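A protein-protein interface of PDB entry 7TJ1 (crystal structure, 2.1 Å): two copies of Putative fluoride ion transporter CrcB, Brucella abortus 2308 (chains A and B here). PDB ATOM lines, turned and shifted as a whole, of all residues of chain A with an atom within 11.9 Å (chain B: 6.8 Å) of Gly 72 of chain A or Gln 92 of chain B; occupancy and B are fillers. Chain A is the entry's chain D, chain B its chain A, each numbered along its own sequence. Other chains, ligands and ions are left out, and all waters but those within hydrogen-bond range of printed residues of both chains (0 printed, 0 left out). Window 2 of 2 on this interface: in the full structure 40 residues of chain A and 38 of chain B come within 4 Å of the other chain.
OG1 of Thr 76 of chain A is in hydrogen-bond range of NH1 of Arg 95 of chain B (2.9 Å).
The side-chain amide nitrogen (NE2) of Gln 92 of chain B sits at hydrogen-bond distance from the backbone carbonyl oxygen (O) of Gly 72 of chain A (2.6 Å).
O of Glu 109 of chain A lies within hydrogen-bond range of NH1 of Arg 95 of chain B, 2.7 Å away.
The backbone carbonyl oxygen (O) of Pro 75 of chain A sits at hydrogen-bond distance from the backbone NH (N) of Glu 109 of chain A, 3.0 Å away.
The backbone carbonyl oxygen (O) of Thr 76 of chain A sits at hydrogen-bond distance from the backbone NH (N) of Gly 63 of chain A (3.0 Å).
N of Leu 71 of chain A sits at hydrogen-bond distance from O of Ala 66 of chain A, 2.8 Å away.
O of Pro 74 of chain A sits at hydrogen-bond distance from OG1 of Thr 76 of chain A, at 2.8 Å.
The backbone NH (N) of His 62 of chain A lies within hydrogen-bond range of the backbone carbonyl oxygen (O) of Thr 76 of chain A (2.9 Å).
His 62 of chain A touches Met 91 of chain B.
Ala 66 of chain A touches Thr 88 of chain B.
CB of Leu 71 of chain A touches CG2 of Thr 88 of chain B, at 3.7 Å.
Leu 73 of chain A touches Arg 95 of chain B (CD1 to NE, 3.8 Å).
CG of Pro 74 of chain A touches NH2 of Arg 95 of chain B, 3.2 Å away.
O of Pro 75 of chain A touches NH1 of Arg 95 of chain B (3.6 Å).
Arg 95 of chain B touches Leu 106 of chain A.
Arg 95 of chain B touches Trp 108 of chain A (CB to CE3, 3.6 Å).
CA of Asp 110 of chain A touches NH2 of Arg 95 of chain B, at 3.7 Å.
Printed residues of chain B within 4 Å of His 62 of chain A: Met 91 (3.4 Å).
Gly 70 of chain A touches none of the printed residues of chain B.
Of chain B, only Gln 92 (2.6 Å) comes within 4 Å of Gly 72 of chain A.
Of the printed residues of chain B, Thr 76 of chain A touches Arg 95 (2.9 Å).
No residue of chain A comes within 4 Å of Asp 93 of chain B.
Of chain A, only Leu 73 (3.8 Å), Pro 74 (3.2 Å), Pro 75 (3.6 Å), Thr 76 (2.9 Å), Leu 106 (3.2 Å), Trp 108 (3.6 Å), Glu 109 (2.7 Å) and Asp 110 (3.7 Å) come within 4 Å of Arg 95 of chain B.
The nearest printed residue of chain A that does not touch Gln 92 of chain B is Leu 73 of chain A (4.02 Å).
The nearest printed residue of chain B that does not touch Leu 106 of chain A is Ile 97 of chain B (5.2 Å).
Of the 22 printed residues of chain A, 12 touch a printed residue of chain B.
Hydrophobic or aromatic side chains of chain A that line the printed part of chain B: His 62, Ala 66, Leu 71, Leu 73, Pro 74, Leu 106 and Trp 108.
Among the printed residues, 12 pairs touch across the chains.
No position is printed for both chains.
Of the 12 pairs that touch across the chains among the printed residues, none has its exchanged pair printed and touching as well.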
ATOM      1  N   ASP A  61       8.357 -20.686  13.926  1.00  0.00           N
ATOM      2  CA  ASP A  61       9.005 -21.902  13.441  1.00  0.00           C
ATOM      3  C   ASP A  61       7.968 -23.017  13.483  1.00  0.00           C
ATOM      4  O   ASP A  61       7.780 -23.684  14.502  1.00  0.00           O
ATOM      5  CB  ASP A  61      10.233 -22.230  14.282  1.00  0.00           C
ATOM      6  CG  ASP A  61      11.083 -23.334  13.674  1.00  0.00           C
ATOM      7  OD1 ASP A  61      10.555 -24.134  12.871  1.00  0.00           O
ATOM      8  OD2 ASP A  61      12.284 -23.404  14.008  1.00  0.00           O
ATOM      9  N   HIS A  62       7.277 -23.214  12.357  1.00  0.00           N
ATOM     10  CA  HIS A  62       6.307 -24.300  12.269  1.00  0.00           C
ATOM     11  C   HIS A  62       6.985 -25.655  12.419  1.00  0.00           C
ATOM     12  O   HIS A  62       6.416 -26.579  13.014  1.00  0.00           O
ATOM     13  CB  HIS A  62       5.548 -24.225  10.944  1.00  0.00           C
ATOM     14  CG  HIS A  62       4.548 -23.114  10.884  1.00  0.00           C
ATOM     15  ND1 HIS A  62       3.636 -22.880  11.890  1.00  0.00           N
ATOM     16  CD2 HIS A  62       4.309 -22.178   9.934  1.00  0.00           C
ATOM     17  CE1 HIS A  62       2.882 -21.845  11.566  1.00  0.00           C
ATOM     18  NE2 HIS A  62       3.270 -21.401  10.384  1.00  0.00           N
ATOM     19  N   GLY A  63       8.201 -25.792  11.887  1.00  0.00           N
ATOM     20  CA  GLY A  63       8.925 -27.046  12.034  1.00  0.00           C
ATOM     21  C   GLY A  63       9.170 -27.408  13.486  1.00  0.00           C
ATOM     22  O   GLY A  63       8.955 -28.550  13.899  1.00  0.00           O
ATOM     23  N   ALA A  64       9.614 -26.432  14.285  1.00  0.00           N
ATOM     24  CA  ALA A  64       9.863 -26.691  15.700  1.00  0.00           C
ATOM     25  C   ALA A  64       8.573 -27.034  16.434  1.00  0.00           C
ATOM     26  O   ALA A  64       8.568 -27.887  17.329  1.00  0.00           O
ATOM     27  CB  ALA A  64      10.543 -25.483  16.347  1.00  0.00           C
ATOM     28  N   GLY A  65       7.469 -26.377  16.072  1.00  0.00           N
ATOM     29  CA  GLY A  65       6.192 -26.704  16.686  1.00  0.00           C
ATOM     30  C   GLY A  65       5.757 -28.128  16.398  1.00  0.00           C
ATOM     31  O   GLY A  65       5.156 -28.789  17.249  1.00  0.00           O
ATOM     32  N   ALA A  66       6.060 -28.622  15.195  1.00  0.00           N
ATOM     33  CA  ALA A  66       5.743 -30.005  14.859  1.00  0.00           C
ATOM     34  C   ALA A  66       6.539 -30.978  15.721  1.00  0.00           C
ATOM     35  O   ALA A  66       6.011 -32.009  16.154  1.00  0.00           O
ATOM     36  CB  ALA A  66       6.011 -30.259  13.377  1.00  0.00           C
ATOM     37  N   LYS A  67       7.811 -30.665  15.984  1.00  0.00           N
ATOM     38  CA  LYS A  67       8.631 -31.547  16.808  1.00  0.00           C
ATOM     39  C   LYS A  67       8.134 -31.580  18.247  1.00  0.00           C
ATOM     40  O   LYS A  67       8.095 -32.646  18.872  1.00  0.00           O
ATOM     41  CB  LYS A  67      10.094 -31.109  16.757  1.00  0.00           C
ATOM     42  CG  LYS A  67      11.029 -32.022  17.541  1.00  0.00           C
ATOM     43  CD  LYS A  67      12.492 -31.674  17.314  1.00  0.00           C
ATOM     44  CE  LYS A  67      13.405 -32.704  17.968  1.00  0.00           C
ATOM     45  NZ  LYS A  67      14.847 -32.424  17.718  1.00  0.00           N
ATOM     46  N   GLU A  68       7.745 -30.422  18.789  1.00  0.00           N
ATOM     47  CA  GLU A  68       7.223 -30.385  20.151  1.00  0.00           C
ATOM     48  C   GLU A  68       5.921 -31.166  20.273  1.00  0.00           C
ATOM     49  O   GLU A  68       5.583 -31.643  21.361  1.00  0.00           O
ATOM     50  CB  GLU A  68       7.018 -28.937  20.597  1.00  0.00           C
ATOM     51  CG  GLU A  68       6.935 -28.767  22.106  1.00  0.00           C
ATOM     52  CD  GLU A  68       8.242 -29.109  22.802  1.00  0.00           C
ATOM     53  OE1 GLU A  68       9.269 -28.468  22.492  1.00  0.00           O
ATOM     54  OE2 GLU A  68       8.246 -30.024  23.654  1.00  0.00           O
ATOM     55  N   ALA A  69       5.184 -31.307  19.173  1.00  0.00           N
ATOM     56  CA  ALA A  69       3.968 -32.105  19.145  1.00  0.00           C
ATOM     57  C   ALA A  69       4.233 -33.580  18.880  1.00  0.00           C
ATOM     58  O   ALA A  69       3.297 -34.385  18.951  1.00  0.00           O
ATOM     59  CB  ALA A  69       3.009 -31.560  18.081  1.00  0.00           C
ATOM     60  N   GLY A  70       5.475 -33.953  18.581  1.00  0.00           N
ATOM     61  CA  GLY A  70       5.783 -35.327  18.236  1.00  0.00           C
ATOM     62  C   GLY A  70       5.432 -35.711  16.819  1.00  0.00           C
ATOM     63  O   GLY A  70       5.213 -36.896  16.545  1.00  0.00           O
ATOM     64  N   LEU A  71       5.369 -34.747  15.906  1.00  0.00           N
ATOM     65  CA  LEU A  71       4.992 -34.991  14.524  1.00  0.00           C
ATOM     66  C   LEU A  71       6.132 -34.605  13.591  1.00  0.00           C
ATOM     67  O   LEU A  71       6.959 -33.746  13.913  1.00  0.00           O
ATOM     68  CB  LEU A  71       3.729 -34.204  14.144  1.00  0.00           C
ATOM     69  CG  LEU A  71       2.418 -34.668  14.781  1.00  0.00           C
ATOM     70  CD1 LEU A  71       1.277 -33.738  14.394  1.00  0.00           C
ATOM     71  CD2 LEU A  71       2.109 -36.098  14.372  1.00  0.00           C
ATOM     72  N   GLY A  72       6.164 -35.250  12.428  1.00  0.00           N
ATOM     73  CA  GLY A  72       7.171 -34.956  11.424  1.00  0.00           C
ATOM     74  C   GLY A  72       6.742 -33.811  10.520  1.00  0.00           C
ATOM     75  O   GLY A  72       5.573 -33.689  10.157  1.00  0.00           O
ATOM     76  N   LEU A  73       7.710 -32.967  10.171  1.00  0.00           N
ATOM     77  CA  LEU A  73       7.515 -31.869   9.234  1.00  0.00           C
ATOM     78  C   LEU A  73       8.879 -31.314   8.843  1.00  0.00           C
ATOM     79  O   LEU A  73       9.698 -31.009   9.719  1.00  0.00           O
ATOM     80  CB  LEU A  73       6.642 -30.767   9.840  1.00  0.00           C
ATOM     81  CG  LEU A  73       6.129 -29.682   8.886  1.00  0.00           C
ATOM     82  CD1 LEU A  73       5.137 -30.259   7.881  1.00  0.00           C
ATOM     83  CD2 LEU A  73       5.502 -28.525   9.654  1.00  0.00           C
ATOM     84  N   PRO A  74       9.165 -31.179   7.551  1.00  0.00           N
ATOM     85  CA  PRO A  74      10.438 -30.584   7.126  1.00  0.00           C
ATOM     86  C   PRO A  74      10.539 -29.142   7.589  1.00  0.00           C
ATOM     87  O   PRO A  74       9.544 -28.566   8.059  1.00  0.00           O
ATOM     88  CB  PRO A  74      10.376 -30.683   5.593  1.00  0.00           C
ATOM     89  CG  PRO A  74       9.389 -31.787   5.321  1.00  0.00           C
ATOM     90  CD  PRO A  74       8.367 -31.659   6.410  1.00  0.00           C
ATOM     91  N   PRO A  75      11.721 -28.529   7.499  1.00  0.00           N
ATOM     92  CA  PRO A  75      11.863 -27.130   7.921  1.00  0.00           C
ATOM     93  C   PRO A  75      10.815 -26.230   7.278  1.00  0.00           C
ATOM     94  O   PRO A  75      10.618 -26.239   6.058  1.00  0.00           O
ATOM     95  CB  PRO A  75      13.280 -26.772   7.464  1.00  0.00           C
ATOM     96  CG  PRO A  75      14.017 -28.072   7.551  1.00  0.00           C
ATOM     97  CD  PRO A  75      13.021 -29.132   7.149  1.00  0.00           C
ATOM     98  N   THR A  76      10.121 -25.467   8.122  1.00  0.00           N
ATOM     99  CA  THR A  76       9.006 -24.622   7.707  1.00  0.00           C
ATOM    100  C   THR A  76       8.944 -23.438   8.658  1.00  0.00           C
ATOM    101  O   THR A  76       8.723 -23.628   9.858  1.00  0.00           O
ATOM    102  CB  THR A  76       7.688 -25.402   7.736  1.00  0.00           C
ATOM    103  OG1 THR A  76       7.817 -26.598   6.957  1.00  0.00           O
ATOM    104  CG2 THR A  76       6.546 -24.557   7.190  1.00  0.00           C
ATOM    105  N   GLU A  77       9.129 -22.225   8.138  1.00  0.00           N
ATOM    106  CA  GLU A  77       9.216 -21.050   8.997  1.00  0.00           C
ATOM    107  C   GLU A  77       8.453 -19.880   8.395  1.00  0.00           C
ATOM    108  O   GLU A  77       8.581 -19.590   7.203  1.00  0.00           O
ATOM    109  CB  GLU A  77      10.677 -20.656   9.242  1.00  0.00           C
ATOM    110  CG  GLU A  77      10.841 -19.538  10.251  1.00  0.00           C
ATOM    111  CD  GLU A  77      12.286 -19.314  10.647  1.00  0.00           C
ATOM    112  OE1 GLU A  77      13.151 -20.113  10.231  1.00  0.00           O
ATOM    113  OE2 GLU A  77      12.554 -18.336  11.377  1.00  0.00           O
ATOM    114  N   LEU A 106       6.386 -17.304   3.976  1.00  0.00           N
ATOM    115  CA  LEU A 106       6.624 -18.663   4.443  1.00  0.00           C
ATOM    116  C   LEU A 106       7.728 -19.292   3.606  1.00  0.00           C
ATOM    117  O   LEU A 106       7.584 -19.432   2.387  1.00  0.00           O
ATOM    118  CB  LEU A 106       5.352 -19.508   4.362  1.00  0.00           C
ATOM    119  CG  LEU A 106       5.509 -20.957   4.836  1.00  0.00           C
ATOM    120  CD1 LEU A 106       5.483 -21.027   6.362  1.00  0.00           C
ATOM    121  CD2 LEU A 106       4.455 -21.873   4.208  1.00  0.00           C
ATOM    122  N   TRP A 108       9.793 -22.832   3.160  1.00  0.00           N
ATOM    123  CA  TRP A 108       9.548 -24.224   3.501  1.00  0.00           C
ATOM    124  C   TRP A 108      10.286 -25.140   2.536  1.00  0.00           C
ATOM    125  O   TRP A 108      10.473 -24.815   1.360  1.00  0.00           O
ATOM    126  CB  TRP A 108       8.044 -24.535   3.513  1.00  0.00           C
ATOM    127  CG  TRP A 108       7.314 -24.193   2.240  1.00  0.00           C
ATOM    128  CD1 TRP A 108       6.924 -22.952   1.824  1.00  0.00           C
ATOM    129  CD2 TRP A 108       6.864 -25.111   1.235  1.00  0.00           C
ATOM    130  NE1 TRP A 108       6.269 -23.039   0.618  1.00  0.00           N
ATOM    131  CE2 TRP A 108       6.218 -24.354   0.235  1.00  0.00           C
ATOM    132  CE3 TRP A 108       6.950 -26.498   1.079  1.00  0.00           C
ATOM    133  CZ2 TRP A 108       5.662 -24.938  -0.903  1.00  0.00           C
ATOM    134  CZ3 TRP A 108       6.393 -27.078  -0.051  1.00  0.00           C
ATOM    135  CH2 TRP A 108       5.759 -26.298  -1.027  1.00  0.00           C
ATOM    136  N   GLU A 109      10.701 -26.292   3.055  1.00  0.00           N
ATOM    137  CA  GLU A 109      11.438 -27.297   2.298  1.00  0.00           C
ATOM    138  C   GLU A 109      10.528 -28.491   2.039  1.00  0.00           C
ATOM    139  O   GLU A 109       9.852 -28.967   2.957  1.00  0.00           O
ATOM    140  CB  GLU A 109      12.692 -27.730   3.064  1.00  0.00           C
ATOM    141  CG  GLU A 109      13.531 -28.796   2.376  1.00  0.00           C
ATOM    142  CD  GLU A 109      14.710 -29.246   3.221  1.00  0.00           C
ATOM    143  OE1 GLU A 109      14.934 -28.660   4.302  1.00  0.00           O
ATOM    144  OE2 GLU A 109      15.412 -30.192   2.806  1.00  0.00           O
ATOM    145  N   ASP A 110      10.501 -28.966   0.794  1.00  0.00           N
ATOM    146  CA  ASP A 110       9.670 -30.112   0.450  1.00  0.00           C
ATOM    147  C   ASP A 110      10.471 -31.402   0.643  1.00  0.00           C
ATOM    148  O   ASP A 110      11.589 -31.394   1.166  1.00  0.00           O
ATOM    149  CB  ASP A 110       9.099 -29.968  -0.966  1.00  0.00           C
ATOM    150  CG  ASP A 110      10.169 -29.942  -2.057  1.00  0.00           C
ATOM    151  OD1 ASP A 110      11.315 -30.377  -1.825  1.00  0.00           O
ATOM    152  OD2 ASP A 110       9.846 -29.479  -3.173  1.00  0.00           O
ATOM    153  N   GLY A 111       9.899 -32.530   0.213  1.00  0.00           N
ATOM    154  CA  GLY A 111      10.541 -33.811   0.447  1.00  0.00           C
ATOM    155  C   GLY A 111      11.790 -34.026  -0.383  1.00  0.00           C
ATOM    156  O   GLY A 111      12.703 -34.739   0.042  1.00  0.00           O
ATOM    157  N   GLY B  87      -2.240 -27.785  13.758  1.00  0.00           N
ATOM    158  CA  GLY B  87      -1.707 -27.071  12.611  1.00  0.00           C
ATOM    159  C   GLY B  87      -0.713 -27.883  11.804  1.00  0.00           C
ATOM    160  O   GLY B  87      -0.607 -27.711  10.586  1.00  0.00           O
ATOM    161  N   THR B  88       0.027 -28.778  12.464  1.00  0.00           N
ATOM    162  CA  THR B  88       1.004 -29.599  11.755  1.00  0.00           C
ATOM    163  C   THR B  88       0.325 -30.546  10.773  1.00  0.00           C
ATOM    164  O   THR B  88       0.800 -30.720   9.644  1.00  0.00           O
ATOM    165  CB  THR B  88       1.856 -30.384  12.752  1.00  0.00           C
ATOM    166  OG1 THR B  88       2.604 -29.473  13.571  1.00  0.00           O
ATOM    167  CG2 THR B  88       2.816 -31.313  12.022  1.00  0.00           C
ATOM    168  N   VAL B  89      -0.785 -31.166  11.183  1.00  0.00           N
ATOM    169  CA  VAL B  89      -1.512 -32.065  10.288  1.00  0.00           C
ATOM    170  C   VAL B  89      -1.985 -31.312   9.051  1.00  0.00           C
ATOM    171  O   VAL B  89      -1.930 -31.832   7.929  1.00  0.00           O
ATOM    172  CB  VAL B  89      -2.686 -32.729  11.033  1.00  0.00           C
ATOM    173  CG1 VAL B  89      -3.454 -33.653  10.100  1.00  0.00           C
ATOM    174  CG2 VAL B  89      -2.182 -33.496  12.244  1.00  0.00           C
ATOM    175  N   LEU B  90      -2.445 -30.073   9.234  1.00  0.00           N
ATOM    176  CA  LEU B  90      -2.857 -29.257   8.096  1.00  0.00           C
ATOM    177  C   LEU B  90      -1.698 -29.021   7.137  1.00  0.00           C
ATOM    178  O   LEU B  90      -1.857 -29.142   5.916  1.00  0.00           O
ATOM    179  CB  LEU B  90      -3.421 -27.922   8.586  1.00  0.00           C
ATOM    180  CG  LEU B  90      -4.714 -27.970   9.402  1.00  0.00           C
ATOM    181  CD1 LEU B  90      -5.091 -26.578   9.863  1.00  0.00           C
ATOM    182  CD2 LEU B  90      -5.839 -28.585   8.581  1.00  0.00           C
ATOM    183  N   MET B  91      -0.525 -28.694   7.670  1.00  0.00           N
ATOM    184  CA  MET B  91       0.624 -28.360   6.843  1.00  0.00           C
ATOM    185  C   MET B  91       1.255 -29.588   6.192  1.00  0.00           C
ATOM    186  O   MET B  91       1.878 -29.478   5.138  1.00  0.00           O
ATOM    187  CB  MET B  91       1.667 -27.607   7.675  1.00  0.00           C
ATOM    188  CG  MET B  91       1.283 -26.161   7.951  1.00  0.00           C
ATOM    189  SD  MET B  91       2.576 -25.195   9.058  1.00  0.00           S
ATOM    190  CE  MET B  91       2.047 -25.863  10.812  1.00  0.00           C
ATOM    191  N   GLN B  92       1.096 -30.755   6.824  1.00  0.00           N
ATOM    192  CA  GLN B  92       1.538 -31.999   6.201  1.00  0.00           C
ATOM    193  C   GLN B  92       0.758 -32.307   4.932  1.00  0.00           C
ATOM    194  O   GLN B  92       1.258 -33.038   4.070  1.00  0.00           O
ATOM    195  CB  GLN B  92       1.397 -33.167   7.180  1.00  0.00           C
ATOM    196  CG  GLN B  92       2.394 -33.160   8.325  1.00  0.00           C
ATOM    197  CD  GLN B  92       2.122 -34.265   9.325  1.00  0.00           C
ATOM    198  OE1 GLN B  92       1.005 -34.775   9.410  1.00  0.00           O
ATOM    199  NE2 GLN B  92       3.143 -34.645  10.083  1.00  0.00           N
ATOM    200  N   ASP B  93      -0.456 -31.772   4.808  1.00  0.00           N
ATOM    201  CA  ASP B  93      -1.256 -31.943   3.600  1.00  0.00           C
ATOM    202  C   ASP B  93      -0.846 -30.931   2.535  1.00  0.00           C
ATOM    203  O   ASP B  93      -0.472 -31.304   1.418  1.00  0.00           O
ATOM    204  CB  ASP B  93      -2.740 -31.803   3.951  1.00  0.00           C
ATOM    205  CG  ASP B  93      -3.656 -32.044   2.768  1.00  0.00           C
ATOM    206  OD1 ASP B  93      -3.177 -32.490   1.706  1.00  0.00           O
ATOM    207  OD2 ASP B  93      -4.870 -31.785   2.906  1.00  0.00           O
ATOM    208  N   LYS B  94      -0.915 -29.644   2.871  1.00  0.00           N
ATOM    209  CA  LYS B  94      -0.507 -28.560   1.980  1.00  0.00           C
ATOM    210  C   LYS B  94       0.308 -27.578   2.809  1.00  0.00           C
ATOM    211  O   LYS B  94      -0.229 -26.943   3.723  1.00  0.00           O
ATOM    212  CB  LYS B  94      -1.716 -27.871   1.347  1.00  0.00           C
ATOM    213  CG  LYS B  94      -2.559 -28.777   0.458  1.00  0.00           C
ATOM    214  CD  LYS B  94      -1.857 -29.057  -0.857  1.00  0.00           C
ATOM    215  CE  LYS B  94      -2.764 -29.810  -1.812  1.00  0.00           C
ATOM    216  NZ  LYS B  94      -2.229 -29.787  -3.201  1.00  0.00           N
ATOM    217  N   ARG B  95       1.600 -27.451   2.498  1.00  0.00           N
ATOM    218  CA  ARG B  95       2.483 -26.660   3.346  1.00  0.00           C
ATOM    219  C   ARG B  95       2.184 -25.170   3.270  1.00  0.00           C
ATOM    220  O   ARG B  95       2.480 -24.447   4.227  1.00  0.00           O
ATOM    221  CB  ARG B  95       3.947 -26.911   2.975  1.00  0.00           C
ATOM    222  CG  ARG B  95       4.933 -26.521   4.064  1.00  0.00           C
ATOM    223  CD  ARG B  95       5.139 -27.664   5.041  1.00  0.00           C
ATOM    224  NE  ARG B  95       5.703 -28.822   4.360  1.00  0.00           N
ATOM    225  CZ  ARG B  95       6.994 -28.975   4.105  1.00  0.00           C
ATOM    226  NH1 ARG B  95       7.885 -28.081   4.500  1.00  0.00           N
ATOM    227  NH2 ARG B  95       7.400 -30.046   3.431  1.00  0.00           N
ATOM    228  N   ILE B  97      -0.427 -23.549   3.673  1.00  0.00           N
ATOM    229  CA  ILE B  97      -1.336 -23.038   4.694  1.00  0.00           C
ATOM    230  C   ILE B  97      -0.565 -22.533   5.910  1.00  0.00           C
ATOM    231  O   ILE B  97      -1.115 -21.779   6.722  1.00  0.00           O
ATOM    232  CB  ILE B  97      -2.378 -24.101   5.095  1.00  0.00           C
ATOM    233  CG1 ILE B  97      -3.545 -23.445   5.845  1.00  0.00           C
ATOM    234  CG2 ILE B  97      -1.741 -25.195   5.939  1.00  0.00           C
ATOM    235  CD1 ILE B  97      -4.680 -24.393   6.174  1.00  0.00           C
ATOM    236  N   SER B 134      -7.164 -35.858   4.148  1.00  0.00           N
ATOM    237  CA  SER B 134      -6.304 -36.107   5.300  1.00  0.00           C
ATOM    238  C   SER B 134      -6.354 -34.971   6.316  1.00  0.00           C
ATOM    239  O   SER B 134      -5.988 -35.177   7.477  1.00  0.00           O
ATOM    240  CB  SER B 134      -4.862 -36.341   4.846  1.00  0.00           C
ATOM    241  OG  SER B 134      -4.316 -35.178   4.248  1.00  0.00           O
ATOM    242  N   SER B 135      -6.807 -33.787   5.912  1.00  0.00           N
ATOM    243  CA  SER B 135      -6.931 -32.644   6.807  1.00  0.00           C
ATOM    244  C   SER B 135      -8.307 -32.526   7.447  1.00  0.00           C
ATOM    245  O   SER B 135      -8.539 -31.571   8.196  1.00  0.00           O
ATOM    246  CB  SER B 135      -6.626 -31.347   6.053  1.00  0.00           C
ATOM    247  OG  SER B 135      -5.301 -31.332   5.566  1.00  0.00           O
